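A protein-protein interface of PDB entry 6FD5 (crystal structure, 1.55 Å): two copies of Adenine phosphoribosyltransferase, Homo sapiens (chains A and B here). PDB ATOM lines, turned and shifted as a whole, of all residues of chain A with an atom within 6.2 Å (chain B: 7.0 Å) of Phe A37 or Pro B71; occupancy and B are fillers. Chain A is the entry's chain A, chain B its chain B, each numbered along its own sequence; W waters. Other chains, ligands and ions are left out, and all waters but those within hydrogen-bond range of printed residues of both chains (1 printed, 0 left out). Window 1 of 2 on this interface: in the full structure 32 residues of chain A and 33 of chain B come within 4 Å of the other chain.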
ATOM      1  N   VAL A   7     -36.970  -2.356 -20.045  1.00  0.00           N
ATOM      2  CA  VAL A   7     -37.615  -1.663 -18.920  1.00  0.00           C
ATOM      3  C   VAL A   7     -38.912  -2.369 -18.539  1.00  0.00           C
ATOM      4  O   VAL A   7     -39.144  -2.680 -17.368  1.00  0.00           O
ATOM      5  CB  VAL A   7     -37.878  -0.165 -19.241  1.00  0.00           C
ATOM      6  CG1 VAL A   7     -38.520   0.560 -18.062  1.00  0.00           C
ATOM      7  CG2 VAL A   7     -36.592   0.554 -19.631  1.00  0.00           C
ATOM      8  N   VAL A  30     -35.910  -2.622 -12.179  1.00  0.00           N
ATOM      9  CA  VAL A  30     -35.259  -1.750 -13.149  1.00  0.00           C
ATOM     10  C   VAL A  30     -33.940  -1.268 -12.552  1.00  0.00           C
ATOM     11  O   VAL A  30     -32.927  -1.213 -13.244  1.00  0.00           O
ATOM     12  CB  VAL A  30     -36.138  -0.519 -13.496  1.00  0.00           C
ATOM     13  CG1 VAL A  30     -35.407   0.446 -14.410  1.00  0.00           C
ATOM     14  CG2 VAL A  30     -37.449  -0.963 -14.141  1.00  0.00           C
ATOM     15  N   LEU A  31     -33.967  -0.928 -11.262  1.00  0.00           N
ATOM     16  CA  LEU A  31     -32.778  -0.418 -10.576  1.00  0.00           C
ATOM     17  C   LEU A  31     -31.718  -1.497 -10.407  1.00  0.00           C
ATOM     18  O   LEU A  31     -30.511  -1.210 -10.423  1.00  0.00           O
ATOM     19  CB  LEU A  31     -33.132   0.142  -9.197  1.00  0.00           C
ATOM     20  CG  LEU A  31     -33.612   1.598  -9.127  1.00  0.00           C
ATOM     21  CD1 LEU A  31     -32.463   2.587  -9.230  1.00  0.00           C
ATOM     22  CD2 LEU A  31     -34.681   1.919 -10.141  1.00  0.00           C
ATOM     23  N   LYS A  32     -32.172  -2.727 -10.182  1.00  0.00           N
ATOM     24  CA  LYS A  32     -31.273  -3.833  -9.876  1.00  0.00           C
ATOM     25  C   LYS A  32     -30.532  -4.372 -11.105  1.00  0.00           C
ATOM     26  O   LYS A  32     -29.475  -4.987 -11.000  1.00  0.00           O
ATOM     27  CB  LYS A  32     -32.053  -4.973  -9.218  1.00  0.00           C
ATOM     28  CG  LYS A  32     -31.193  -6.170  -8.855  1.00  0.00           C
ATOM     29  CD  LYS A  32     -31.963  -7.197  -8.045  1.00  0.00           C
ATOM     30  CE  LYS A  32     -31.043  -8.311  -7.591  1.00  0.00           C
ATOM     31  NZ  LYS A  32     -31.749  -9.394  -6.842  1.00  0.00           N
ATOM     32  N   ASP A  33     -31.126  -4.172 -12.275  1.00  0.00           N
ATOM     33  CA  ASP A  33     -30.546  -4.625 -13.525  1.00  0.00           C
ATOM     34  C   ASP A  33     -29.915  -3.413 -14.235  1.00  0.00           C
ATOM     35  O   ASP A  33     -30.623  -2.531 -14.735  1.00  0.00           O
ATOM     36  CB  ASP A  33     -31.661  -5.228 -14.377  1.00  0.00           C
ATOM     37  CG  ASP A  33     -31.188  -5.673 -15.741  1.00  0.00           C
ATOM     38  OD1 ASP A  33     -30.044  -5.367 -16.118  1.00  0.00           O
ATOM     39  OD2 ASP A  33     -31.985  -6.326 -16.451  1.00  0.00           O
ATOM     40  N   PRO A  34     -28.583  -3.317 -14.217  1.00  0.00           N
ATOM     41  CA  PRO A  34     -27.967  -2.079 -14.709  1.00  0.00           C
ATOM     42  C   PRO A  34     -28.266  -1.764 -16.175  1.00  0.00           C
ATOM     43  O   PRO A  34     -28.301  -0.597 -16.558  1.00  0.00           O
ATOM     44  CB  PRO A  34     -26.471  -2.296 -14.458  1.00  0.00           C
ATOM     45  CG  PRO A  34     -26.302  -3.777 -14.347  1.00  0.00           C
ATOM     46  CD  PRO A  34     -27.585  -4.308 -13.783  1.00  0.00           C
ATOM     47  N   ALA A  35     -28.549  -2.782 -16.979  1.00  0.00           N
ATOM     48  CA  ALA A  35     -28.917  -2.547 -18.378  1.00  0.00           C
ATOM     49  C   ALA A  35     -30.318  -1.936 -18.494  1.00  0.00           C
ATOM     50  O   ALA A  35     -30.567  -1.111 -19.374  1.00  0.00           O
ATOM     51  CB  ALA A  35     -28.829  -3.836 -19.177  1.00  0.00           C
ATOM     52  N   SER A  36     -31.219  -2.356 -17.611  1.00  0.00           N
ATOM     53  CA  SER A  36     -32.577  -1.830 -17.570  1.00  0.00           C
ATOM     54  C   SER A  36     -32.554  -0.364 -17.149  1.00  0.00           C
ATOM     55  O   SER A  36     -33.220   0.479 -17.732  1.00  0.00           O
ATOM     56  CB  SER A  36     -33.433  -2.656 -16.601  1.00  0.00           C
ATOM     57  OG  SER A  36     -34.807  -2.288 -16.625  1.00  0.00           O
ATOM     58  N   PHE A  37     -31.789  -0.062 -16.113  1.00  0.00           N
ATOM     59  CA  PHE A  37     -31.738   1.298 -15.606  1.00  0.00           C
ATOM     60  C   PHE A  37     -31.143   2.214 -16.670  1.00  0.00           C
ATOM     61  O   PHE A  37     -31.669   3.289 -16.938  1.00  0.00           O
ATOM     62  CB  PHE A  37     -30.898   1.363 -14.332  1.00  0.00           C
ATOM     63  CG  PHE A  37     -30.855   2.737 -13.706  1.00  0.00           C
ATOM     64  CD1 PHE A  37     -31.950   3.224 -13.007  1.00  0.00           C
ATOM     65  CD2 PHE A  37     -29.727   3.531 -13.814  1.00  0.00           C
ATOM     66  CE1 PHE A  37     -31.927   4.493 -12.440  1.00  0.00           C
ATOM     67  CE2 PHE A  37     -29.701   4.806 -13.258  1.00  0.00           C
ATOM     68  CZ  PHE A  37     -30.793   5.282 -12.565  1.00  0.00           C
ATOM     69  N   ARG A  38     -30.046   1.785 -17.280  1.00  0.00           N
ATOM     70  CA  ARG A  38     -29.426   2.540 -18.370  1.00  0.00           C
ATOM     71  C   ARG A  38     -30.413   2.793 -19.521  1.00  0.00           C
ATOM     72  O   ARG A  38     -30.468   3.899 -20.086  1.00  0.00           O
ATOM     73  CB  ARG A  38     -28.199   1.780 -18.874  1.00  0.00           C
ATOM     74  CG  ARG A  38     -27.209   2.611 -19.667  1.00  0.00           C
ATOM     75  CD  ARG A  38     -25.822   1.982 -19.629  1.00  0.00           C
ATOM     76  NE  ARG A  38     -25.867   0.525 -19.757  1.00  0.00           N
ATOM     77  CZ  ARG A  38     -25.397  -0.331 -18.852  1.00  0.00           C
ATOM     78  NH1 ARG A  38     -25.490  -1.636 -19.067  1.00  0.00           N
ATOM     79  NH2 ARG A  38     -24.827   0.110 -17.736  1.00  0.00           N
ATOM     80  N   ALA A  39     -31.194   1.775 -19.877  1.00  0.00           N
ATOM     81  CA  ALA A  39     -32.218   1.921 -20.904  1.00  0.00           C
ATOM     82  C   ALA A  39     -33.258   2.978 -20.526  1.00  0.00           C
ATOM     83  O   ALA A  39     -33.651   3.799 -21.346  1.00  0.00           O
ATOM     84  CB  ALA A  39     -32.900   0.589 -21.163  1.00  0.00           C
ATOM     85  N   ALA A  40     -33.738   2.934 -19.288  1.00  0.00           N
ATOM     86  CA  ALA A  40     -34.782   3.853 -18.866  1.00  0.00           C
ATOM     87  C   ALA A  40     -34.271   5.282 -18.967  1.00  0.00           C
ATOM     88  O   ALA A  40     -34.961   6.156 -19.493  1.00  0.00           O
ATOM     89  CB  ALA A  40     -35.223   3.542 -17.448  1.00  0.00           C
ATOM     90  N   ILE A  41     -33.090   5.531 -18.400  1.00  0.00           N
ATOM     91  CA  ILE A  41     -32.500   6.867 -18.424  1.00  0.00           C
ATOM     92  C   ILE A  41     -32.262   7.312 -19.863  1.00  0.00           C
ATOM     93  O   ILE A  41     -32.581   8.441 -20.217  1.00  0.00           O
ATOM     94  CB  ILE A  41     -31.172   6.932 -17.639  1.00  0.00           C
ATOM     95  CG1 ILE A  41     -31.402   6.608 -16.157  1.00  0.00           C
ATOM     96  CG2 ILE A  41     -30.520   8.304 -17.758  1.00  0.00           C
ATOM     97  CD1 ILE A  41     -32.381   7.532 -15.469  1.00  0.00           C
ATOM     98  N   GLY A  42     -31.748   6.423 -20.711  1.00  0.00           N
ATOM     99  CA  GLY A  42     -31.468   6.814 -22.082  1.00  0.00           C
ATOM    100  C   GLY A  42     -32.704   7.182 -22.874  1.00  0.00           C
ATOM    101  O   GLY A  42     -32.669   8.091 -23.709  1.00  0.00           O
ATOM    102  N   PHE A  67     -36.182  10.573  -6.930  1.00  0.00           N
ATOM    103  CA  PHE A  67     -34.767  10.719  -6.583  1.00  0.00           C
ATOM    104  C   PHE A  67     -33.902   9.643  -7.239  1.00  0.00           C
ATOM    105  O   PHE A  67     -32.702   9.830  -7.416  1.00  0.00           O
ATOM    106  CB  PHE A  67     -34.556  10.618  -5.066  1.00  0.00           C
ATOM    107  CG  PHE A  67     -35.010  11.819  -4.274  1.00  0.00           C
ATOM    108  CD1 PHE A  67     -35.638  12.896  -4.871  1.00  0.00           C
ATOM    109  CD2 PHE A  67     -34.823  11.833  -2.908  1.00  0.00           C
ATOM    110  CE1 PHE A  67     -36.051  13.977  -4.117  1.00  0.00           C
ATOM    111  CE2 PHE A  67     -35.221  12.921  -2.144  1.00  0.00           C
ATOM    112  CZ  PHE A  67     -35.842  13.986  -2.751  1.00  0.00           C
ATOM    113  N   LEU A  68     -34.502   8.483  -7.495  1.00  0.00           N
ATOM    114  CA  LEU A  68     -33.778   7.362  -8.102  1.00  0.00           C
ATOM    115  C   LEU A  68     -33.414   7.649  -9.553  1.00  0.00           C
ATOM    116  O   LEU A  68     -32.450   7.087 -10.074  1.00  0.00           O
ATOM    117  CB  LEU A  68     -34.603   6.078  -8.058  1.00  0.00           C
ATOM    118  CG  LEU A  68     -34.852   5.479  -6.674  1.00  0.00           C
ATOM    119  CD1 LEU A  68     -35.945   4.424  -6.720  1.00  0.00           C
ATOM    120  CD2 LEU A  68     -33.596   4.881  -6.079  1.00  0.00           C
ATOM    121  N   PHE A  69     -34.223   8.478 -10.208  1.00  0.00           N
ATOM    122  CA  PHE A  69     -34.033   8.762 -11.619  1.00  0.00           C
ATOM    123  C   PHE A  69     -33.521  10.169 -11.914  1.00  0.00           C
ATOM    124  O   PHE A  69     -32.766  10.358 -12.871  1.00  0.00           O
ATOM    125  CB  PHE A  69     -35.333   8.495 -12.366  1.00  0.00           C
ATOM    126  CG  PHE A  69     -35.804   7.074 -12.230  1.00  0.00           C
ATOM    127  CD1 PHE A  69     -35.254   6.080 -13.026  1.00  0.00           C
ATOM    128  CD2 PHE A  69     -36.731   6.717 -11.260  1.00  0.00           C
ATOM    129  CE1 PHE A  69     -35.634   4.754 -12.873  1.00  0.00           C
ATOM    130  CE2 PHE A  69     -37.116   5.396 -11.110  1.00  0.00           C
ATOM    131  CZ  PHE A  69     -36.575   4.419 -11.921  1.00  0.00           C
ATOM    132  N   SER A  72     -29.486  10.801 -12.273  1.00  0.00           N
ATOM    133  CA  SER A  72     -28.890  10.143 -13.442  1.00  0.00           C
ATOM    134  C   SER A  72     -29.384  10.742 -14.761  1.00  0.00           C
ATOM    135  O   SER A  72     -28.618  10.872 -15.712  1.00  0.00           O
ATOM    136  CB  SER A  72     -29.154   8.640 -13.425  1.00  0.00           C
ATOM    137  OG  SER A  72     -28.520   8.038 -12.310  1.00  0.00           O
ATOM    138  N   ILE B  41     -19.582  11.286  -7.287  1.00  0.00           N
ATOM    139  CA  ILE B  41     -19.775   9.909  -7.717  1.00  0.00           C
ATOM    140  C   ILE B  41     -18.434   9.277  -8.108  1.00  0.00           C
ATOM    141  O   ILE B  41     -18.161   8.142  -7.751  1.00  0.00           O
ATOM    142  CB  ILE B  41     -20.750   9.807  -8.891  1.00  0.00           C
ATOM    143  CG1 ILE B  41     -22.138  10.289  -8.469  1.00  0.00           C
ATOM    144  CG2 ILE B  41     -20.776   8.371  -9.439  1.00  0.00           C
ATOM    145  CD1 ILE B  41     -22.755   9.509  -7.330  1.00  0.00           C
ATOM    146  N   ILE B  59     -24.828  -2.334  -5.227  1.00  0.00           N
ATOM    147  CA  ILE B  59     -24.959  -1.188  -4.309  1.00  0.00           C
ATOM    148  C   ILE B  59     -26.336  -1.265  -3.657  1.00  0.00           C
ATOM    149  O   ILE B  59     -27.298  -1.685  -4.293  1.00  0.00           O
ATOM    150  CB  ILE B  59     -24.799   0.134  -5.088  1.00  0.00           C
ATOM    151  CG1 ILE B  59     -23.414   0.206  -5.732  1.00  0.00           C
ATOM    152  CG2 ILE B  59     -25.059   1.347  -4.212  1.00  0.00           C
ATOM    153  CD1 ILE B  59     -22.259   0.094  -4.769  1.00  0.00           C
ATOM    154  N   GLY B  61     -28.948   1.337  -1.810  1.00  0.00           N
ATOM    155  CA  GLY B  61     -29.206   2.745  -1.503  1.00  0.00           C
ATOM    156  C   GLY B  61     -30.266   2.877  -0.437  1.00  0.00           C
ATOM    157  O   GLY B  61     -31.259   2.160  -0.466  1.00  0.00           O
ATOM    158  N   GLY B  66     -30.210   8.702   0.177  1.00  0.00           N
ATOM    159  CA  GLY B  66     -29.294   7.736  -0.409  1.00  0.00           C
ATOM    160  C   GLY B  66     -29.694   7.319  -1.819  1.00  0.00           C
ATOM    161  O   GLY B  66     -28.867   6.860  -2.611  1.00  0.00           O
ATOM    162  N   PHE B  67     -30.987   7.435  -2.111  1.00  0.00           N
ATOM    163  CA  PHE B  67     -31.493   7.189  -3.449  1.00  0.00           C
ATOM    164  C   PHE B  67     -30.908   8.155  -4.474  1.00  0.00           C
ATOM    165  O   PHE B  67     -30.883   7.872  -5.654  1.00  0.00           O
ATOM    166  CB  PHE B  67     -33.019   7.343  -3.500  1.00  0.00           C
ATOM    167  CG  PHE B  67     -33.797   6.240  -2.836  1.00  0.00           C
ATOM    168  CD1 PHE B  67     -33.178   5.148  -2.233  1.00  0.00           C
ATOM    169  CD2 PHE B  67     -35.184   6.274  -2.890  1.00  0.00           C
ATOM    170  CE1 PHE B  67     -33.936   4.142  -1.659  1.00  0.00           C
ATOM    171  CE2 PHE B  67     -35.945   5.273  -2.313  1.00  0.00           C
ATOM    172  CZ  PHE B  67     -35.319   4.192  -1.720  1.00  0.00           C
ATOM    173  N   LEU B  68     -30.453   9.305  -4.016  1.00  0.00           N
ATOM    174  CA  LEU B  68     -29.905  10.299  -4.937  1.00  0.00           C
ATOM    175  C   LEU B  68     -28.533   9.882  -5.458  1.00  0.00           C
ATOM    176  O   LEU B  68     -28.101  10.357  -6.502  1.00  0.00           O
ATOM    177  CB  LEU B  68     -29.761  11.651  -4.238  1.00  0.00           C
ATOM    178  CG  LEU B  68     -31.056  12.373  -3.884  1.00  0.00           C
ATOM    179  CD1 LEU B  68     -30.806  13.435  -2.815  1.00  0.00           C
ATOM    180  CD2 LEU B  68     -31.715  12.986  -5.109  1.00  0.00           C
ATOM    181  N   PHE B  69     -27.841   9.032  -4.709  1.00  0.00           N
ATOM    182  CA  PHE B  69     -26.455   8.683  -5.035  1.00  0.00           C
ATOM    183  C   PHE B  69     -26.287   7.229  -5.452  1.00  0.00           C
ATOM    184  O   PHE B  69     -25.427   6.909  -6.276  1.00  0.00           O
ATOM    185  CB  PHE B  69     -25.545   8.982  -3.844  1.00  0.00           C
ATOM    186  CG  PHE B  69     -25.485  10.431  -3.503  1.00  0.00           C
ATOM    187  CD1 PHE B  69     -24.646  11.277  -4.194  1.00  0.00           C
ATOM    188  CD2 PHE B  69     -26.351  10.969  -2.558  1.00  0.00           C
ATOM    189  CE1 PHE B  69     -24.642  12.641  -3.933  1.00  0.00           C
ATOM    190  CE2 PHE B  69     -26.345  12.322  -2.287  1.00  0.00           C
ATOM    191  CZ  PHE B  69     -25.491  13.160  -2.973  1.00  0.00           C
ATOM    192  N   GLY B  70     -27.104   6.346  -4.882  1.00  0.00           N
ATOM    193  CA  GLY B  70     -26.974   4.902  -5.141  1.00  0.00           C
ATOM    194  C   GLY B  70     -26.971   4.498  -6.610  1.00  0.00           C
ATOM    195  O   GLY B  70     -26.047   3.796  -7.076  1.00  0.00           O
ATOM    196  N   PRO B  71     -28.033   4.864  -7.351  1.00  0.00           N
ATOM    197  CA  PRO B  71     -28.096   4.433  -8.747  1.00  0.00           C
ATOM    198  C   PRO B  71     -26.968   4.980  -9.612  1.00  0.00           C
ATOM    199  O   PRO B  71     -26.401   4.247 -10.428  1.00  0.00           O
ATOM    200  CB  PRO B  71     -29.465   4.958  -9.214  1.00  0.00           C
ATOM    201  CG  PRO B  71     -30.263   5.028  -7.963  1.00  0.00           C
ATOM    202  CD  PRO B  71     -29.303   5.470  -6.911  1.00  0.00           C
ATOM    203  N   SER B  72     -26.573   6.233  -9.401  1.00  0.00           N
ATOM    204  CA  SER B  72     -25.478   6.772 -10.186  1.00  0.00           C
ATOM    205  C   SER B  72     -24.161   6.092  -9.854  1.00  0.00           C
ATOM    206  O   SER B  72     -23.350   5.852 -10.736  1.00  0.00           O
ATOM    207  CB  SER B  72     -25.348   8.272  -9.971  1.00  0.00           C
ATOM    208  OG  SER B  72     -26.426   8.965 -10.584  1.00  0.00           O
ATOM    209  N   LEU B  73     -23.954   5.787  -8.571  1.00  0.00           N
ATOM    210  CA  LEU B  73     -22.730   5.095  -8.139  1.00  0.00           C
ATOM    211  C   LEU B  73     -22.701   3.679  -8.741  1.00  0.00           C
ATOM    212  O   LEU B  73     -21.684   3.222  -9.310  1.00  0.00           O
ATOM    213  CB  LEU B  73     -22.676   5.034  -6.615  1.00  0.00           C
ATOM    214  CG  LEU B  73     -21.452   4.371  -5.985  1.00  0.00           C
ATOM    215  CD1 LEU B  73     -20.150   4.930  -6.544  1.00  0.00           C
ATOM    216  CD2 LEU B  73     -21.512   4.564  -4.477  1.00  0.00           C
ATOM    217  N   ALA B  74     -23.832   2.982  -8.620  1.00  0.00           N
ATOM    218  CA  ALA B  74     -23.941   1.648  -9.204  1.00  0.00           C
ATOM    219  C   ALA B  74     -23.649   1.669 -10.707  1.00  0.00           C
ATOM    220  O   ALA B  74     -22.880   0.845 -11.204  1.00  0.00           O
ATOM    221  CB  ALA B  74     -25.321   1.058  -8.914  1.00  0.00           C
ATOM    222  N   GLN B  75     -24.254   2.610 -11.423  1.00  0.00           N
ATOM    223  CA  GLN B  75     -24.048   2.730 -12.863  1.00  0.00           C
ATOM    224  C   GLN B  75     -22.579   2.934 -13.197  1.00  0.00           C
ATOM    225  O   GLN B  75     -22.046   2.304 -14.122  1.00  0.00           O
ATOM    226  CB  GLN B  75     -24.909   3.871 -13.410  1.00  0.00           C
ATOM    227  CG  GLN B  75     -26.342   3.441 -13.702  1.00  0.00           C
ATOM    228  CD  GLN B  75     -26.462   2.594 -14.970  1.00  0.00           C
ATOM    229  OE1 GLN B  75     -26.146   3.056 -16.064  1.00  0.00           O
ATOM    230  NE2 GLN B  75     -26.909   1.357 -14.825  1.00  0.00           N
ATOM    231  N   GLU B  76     -21.901   3.770 -12.415  1.00  0.00           N
ATOM    232  CA  GLU B  76     -20.491   4.048 -12.670  1.00  0.00           C
ATOM    233  C   GLU B  76     -19.630   2.796 -12.478  1.00  0.00           C
ATOM    234  O   GLU B  76     -18.618   2.631 -13.148  1.00  0.00           O
ATOM    235  CB  GLU B  76     -20.009   5.208 -11.795  1.00  0.00           C
ATOM    236  CG  GLU B  76     -18.529   5.543 -11.930  1.00  0.00           C
ATOM    237  CD  GLU B  76     -18.153   6.105 -13.286  1.00  0.00           C
ATOM    238  OE1 GLU B  76     -19.032   6.663 -13.967  1.00  0.00           O
ATOM    239  OE2 GLU B  76     -16.969   5.969 -13.676  1.00  0.00           O
ATOM    240  N   LEU B  77     -20.051   1.897 -11.584  1.00  0.00           N
ATOM    241  CA  LEU B  77     -19.324   0.643 -11.317  1.00  0.00           C
ATOM    242  C   LEU B  77     -19.776  -0.535 -12.194  1.00  0.00           C
ATOM    243  O   LEU B  77     -19.241  -1.651 -12.082  1.00  0.00           O
ATOM    244  CB  LEU B  77     -19.497   0.264  -9.845  1.00  0.00           C
ATOM    245  CG  LEU B  77     -18.881   1.222  -8.819  1.00  0.00           C
ATOM    246  CD1 LEU B  77     -19.365   0.924  -7.409  1.00  0.00           C
ATOM    247  CD2 LEU B  77     -17.367   1.147  -8.907  1.00  0.00           C
ATOM    248  N   LEU B  79     -22.853  -1.861 -12.011  1.00  0.00           N
ATOM    249  CA  LEU B  79     -23.599  -2.718 -11.091  1.00  0.00           C
ATOM    250  C   LEU B  79     -25.037  -2.275 -10.964  1.00  0.00           C
ATOM    251  O   LEU B  79     -25.348  -1.129 -11.267  1.00  0.00           O
ATOM    252  CB  LEU B  79     -22.981  -2.664  -9.697  1.00  0.00           C
ATOM    253  CG  LEU B  79     -21.523  -3.094  -9.576  1.00  0.00           C
ATOM    254  CD1 LEU B  79     -21.083  -2.957  -8.133  1.00  0.00           C
ATOM    255  CD2 LEU B  79     -21.347  -4.520 -10.045  1.00  0.00           C
ATOM    256  N   GLY B  80     -25.888  -3.177 -10.464  1.00  0.00           N
ATOM    257  CA  GLY B  80     -27.249  -2.822 -10.093  1.00  0.00           C
ATOM    258  C   GLY B  80     -27.328  -2.216  -8.703  1.00  0.00           C
ATOM    259  O   GLY B  80     -26.349  -2.236  -7.932  1.00  0.00           O
ATOM    260  N   CYS B  81     -28.489  -1.640  -8.385  1.00  0.00           N
ATOM    261  CA  CYS B  81     -28.729  -0.990  -7.100  1.00  0.00           C
ATOM    262  C   CYS B  81     -29.973  -1.612  -6.484  1.00  0.00           C
ATOM    263  O   CYS B  81     -31.019  -1.716  -7.158  1.00  0.00           O
ATOM    264  CB  CYS B  81     -28.939   0.512  -7.304  1.00  0.00           C
ATOM    265  SG  CYS B  81     -29.034   1.451  -5.765  1.00  0.00           S
ATOM    266  N   LEU B  83     -32.712  -1.579  -3.080  1.00  0.00           N
ATOM    267  CA  LEU B  83     -33.314  -0.508  -2.266  1.00  0.00           C
ATOM    268  C   LEU B  83     -33.635  -0.968  -0.867  1.00  0.00           C
ATOM    269  O   LEU B  83     -34.189  -2.046  -0.686  1.00  0.00           O
ATOM    270  CB  LEU B  83     -34.612  -0.003  -2.901  1.00  0.00           C
ATOM    271  CG  LEU B  83     -34.528   0.417  -4.366  1.00  0.00           C
ATOM    272  CD1 LEU B  83     -35.904   0.877  -4.811  1.00  0.00           C
ATOM    273  CD2 LEU B  83     -33.485   1.505  -4.560  1.00  0.00           C
ATOM    274  N   VAL B 124     -24.888   2.712   0.612  1.00  0.00           N
ATOM    275  CA  VAL B 124     -24.618   4.134   0.464  1.00  0.00           C
ATOM    276  C   VAL B 124     -25.753   5.007   0.950  1.00  0.00           C
ATOM    277  O   VAL B 124     -26.930   4.731   0.726  1.00  0.00           O
ATOM    278  CB  VAL B 124     -24.270   4.529  -0.975  1.00  0.00           C
ATOM    279  CG1 VAL B 124     -25.469   4.311  -1.886  1.00  0.00           C
ATOM    280  CG2 VAL B 124     -23.802   5.982  -1.032  1.00  0.00           C
HETATM  281  O   HOH W   1     -22.899   0.831 -16.384  1.00  0.00           O
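N of Cys B81 lies within hydrogen-bond range of O of Leu A31, at 2.9 Å.
The backbone NH of Lys A32 sits at hydrogen-bond distance from the backbone carbonyl oxygen of Cys B81, at 3.4 Å.
The backbone carbonyl oxygen of Pro A34 sits at hydrogen-bond distance from the side-chain amide nitrogen of Gln B75, 3.0 Å away.
The side-chain hydroxyl (OG) of Ser B72 is in hydrogen-bond range of the side-chain hydroxyl (OG) of Ser A72 (2.9 Å).
The backbone carbonyl oxygen (O) of Phe B67 lies close to the backbone carbonyl oxygen (O) of Phe A67, at 3.2 Å.
The backbone carbonyl oxygen (O) of Val A30 sits at hydrogen-bond distance from the backbone NH (N) of Phe A37, 3.3 Å away.
The backbone carbonyl oxygen of Gly B80 is in hydrogen-bond range of the backbone NH of Ile B59 (3.1 Å).
O of Ala B74 sits at hydrogen-bond distance from N of Leu B79 (2.8 Å).
Among the printed residues, pairs that only touch across the chains: Leu A31 with Pro B71, Leu A31 with Gly B80, Lys A32 with Gly B80, Pro A34 with Leu B79, Pro A34 with Gly B80, Phe A37 with Pro B71, Phe A37 with Gln B75, Arg A38 with Gln B75, Phe A67 with Leu B68, Leu A68 with Phe B67, Leu A68 with Pro B71 and Leu A68 with Leu B83.
Phe A37 touches just these residues of chain B: Pro B71 and Gln B75.
Of the printed residues of chain A, Pro B71 touches Leu A31 (3.5 Å), Phe A37 (3.6 Å) and Leu A68 (3.7 Å).
Of the printed residues of chain A, Phe B67 touches Phe A67 and Leu A68.
Printed residues of chain B within 4 Å of Pro A34: Gln B75 (3.0 Å), Leu B79 (3.6 Å) and Gly B80 (3.9 Å).
Printed residues of chain B within 4 Å of Ser A72: Ser B72.
Printed residues of chain A within 4 Å of Gly B80: Leu A31 (3.7 Å), Lys A32 (3.2 Å) and Pro A34 (3.9 Å).
Printed residues of chain A within 4 Å of Cys B81: Leu A31 and Lys A32.
Val A7 touches none of the printed residues of chain B.
The nearest residue of chain B that does not touch Phe A37 is Ser B72 (5.2 Å).
The nearest residue of chain A that does not touch Pro B71 is Ser A72 (4.4 Å).
The nearest printed residue of chain B that does not touch Leu A68 is Leu B68 (5.4 Å).
Hydrophobic or aromatic side chains of chain A that line the printed part of chain B: Leu A31, Pro A34, Phe A37, Phe A67 and Leu A68.
Printed residues of chain B that touch a printed residue of chain A: Phe B67, Leu B68, Pro B71, Ser B72, Gln B75, Leu B79, Gly B80, Cys B81 and Leu B83.
Hydrophobic or aromatic side chains of chain B within 4 Å of the printed part of chain A: Phe B67, Leu B68, Pro B71 and Leu B83.
Phe A67 touches its own counterpart, Phe B67.
Phe A67 touches Leu B68, and with the chains exchanged Leu A68 touches Phe B67.
Ser A72 touches its own counterpart, Ser B72.
Of the 17 pairs that touch across the chains among the printed residues, 4 have their exchanged pair printed and touching as well.
Water W1 bridges the guanidinium group of Arg A38 (2.5 Å) and the backbone carbonyl oxygen of Gln B75 (2.8 Å).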
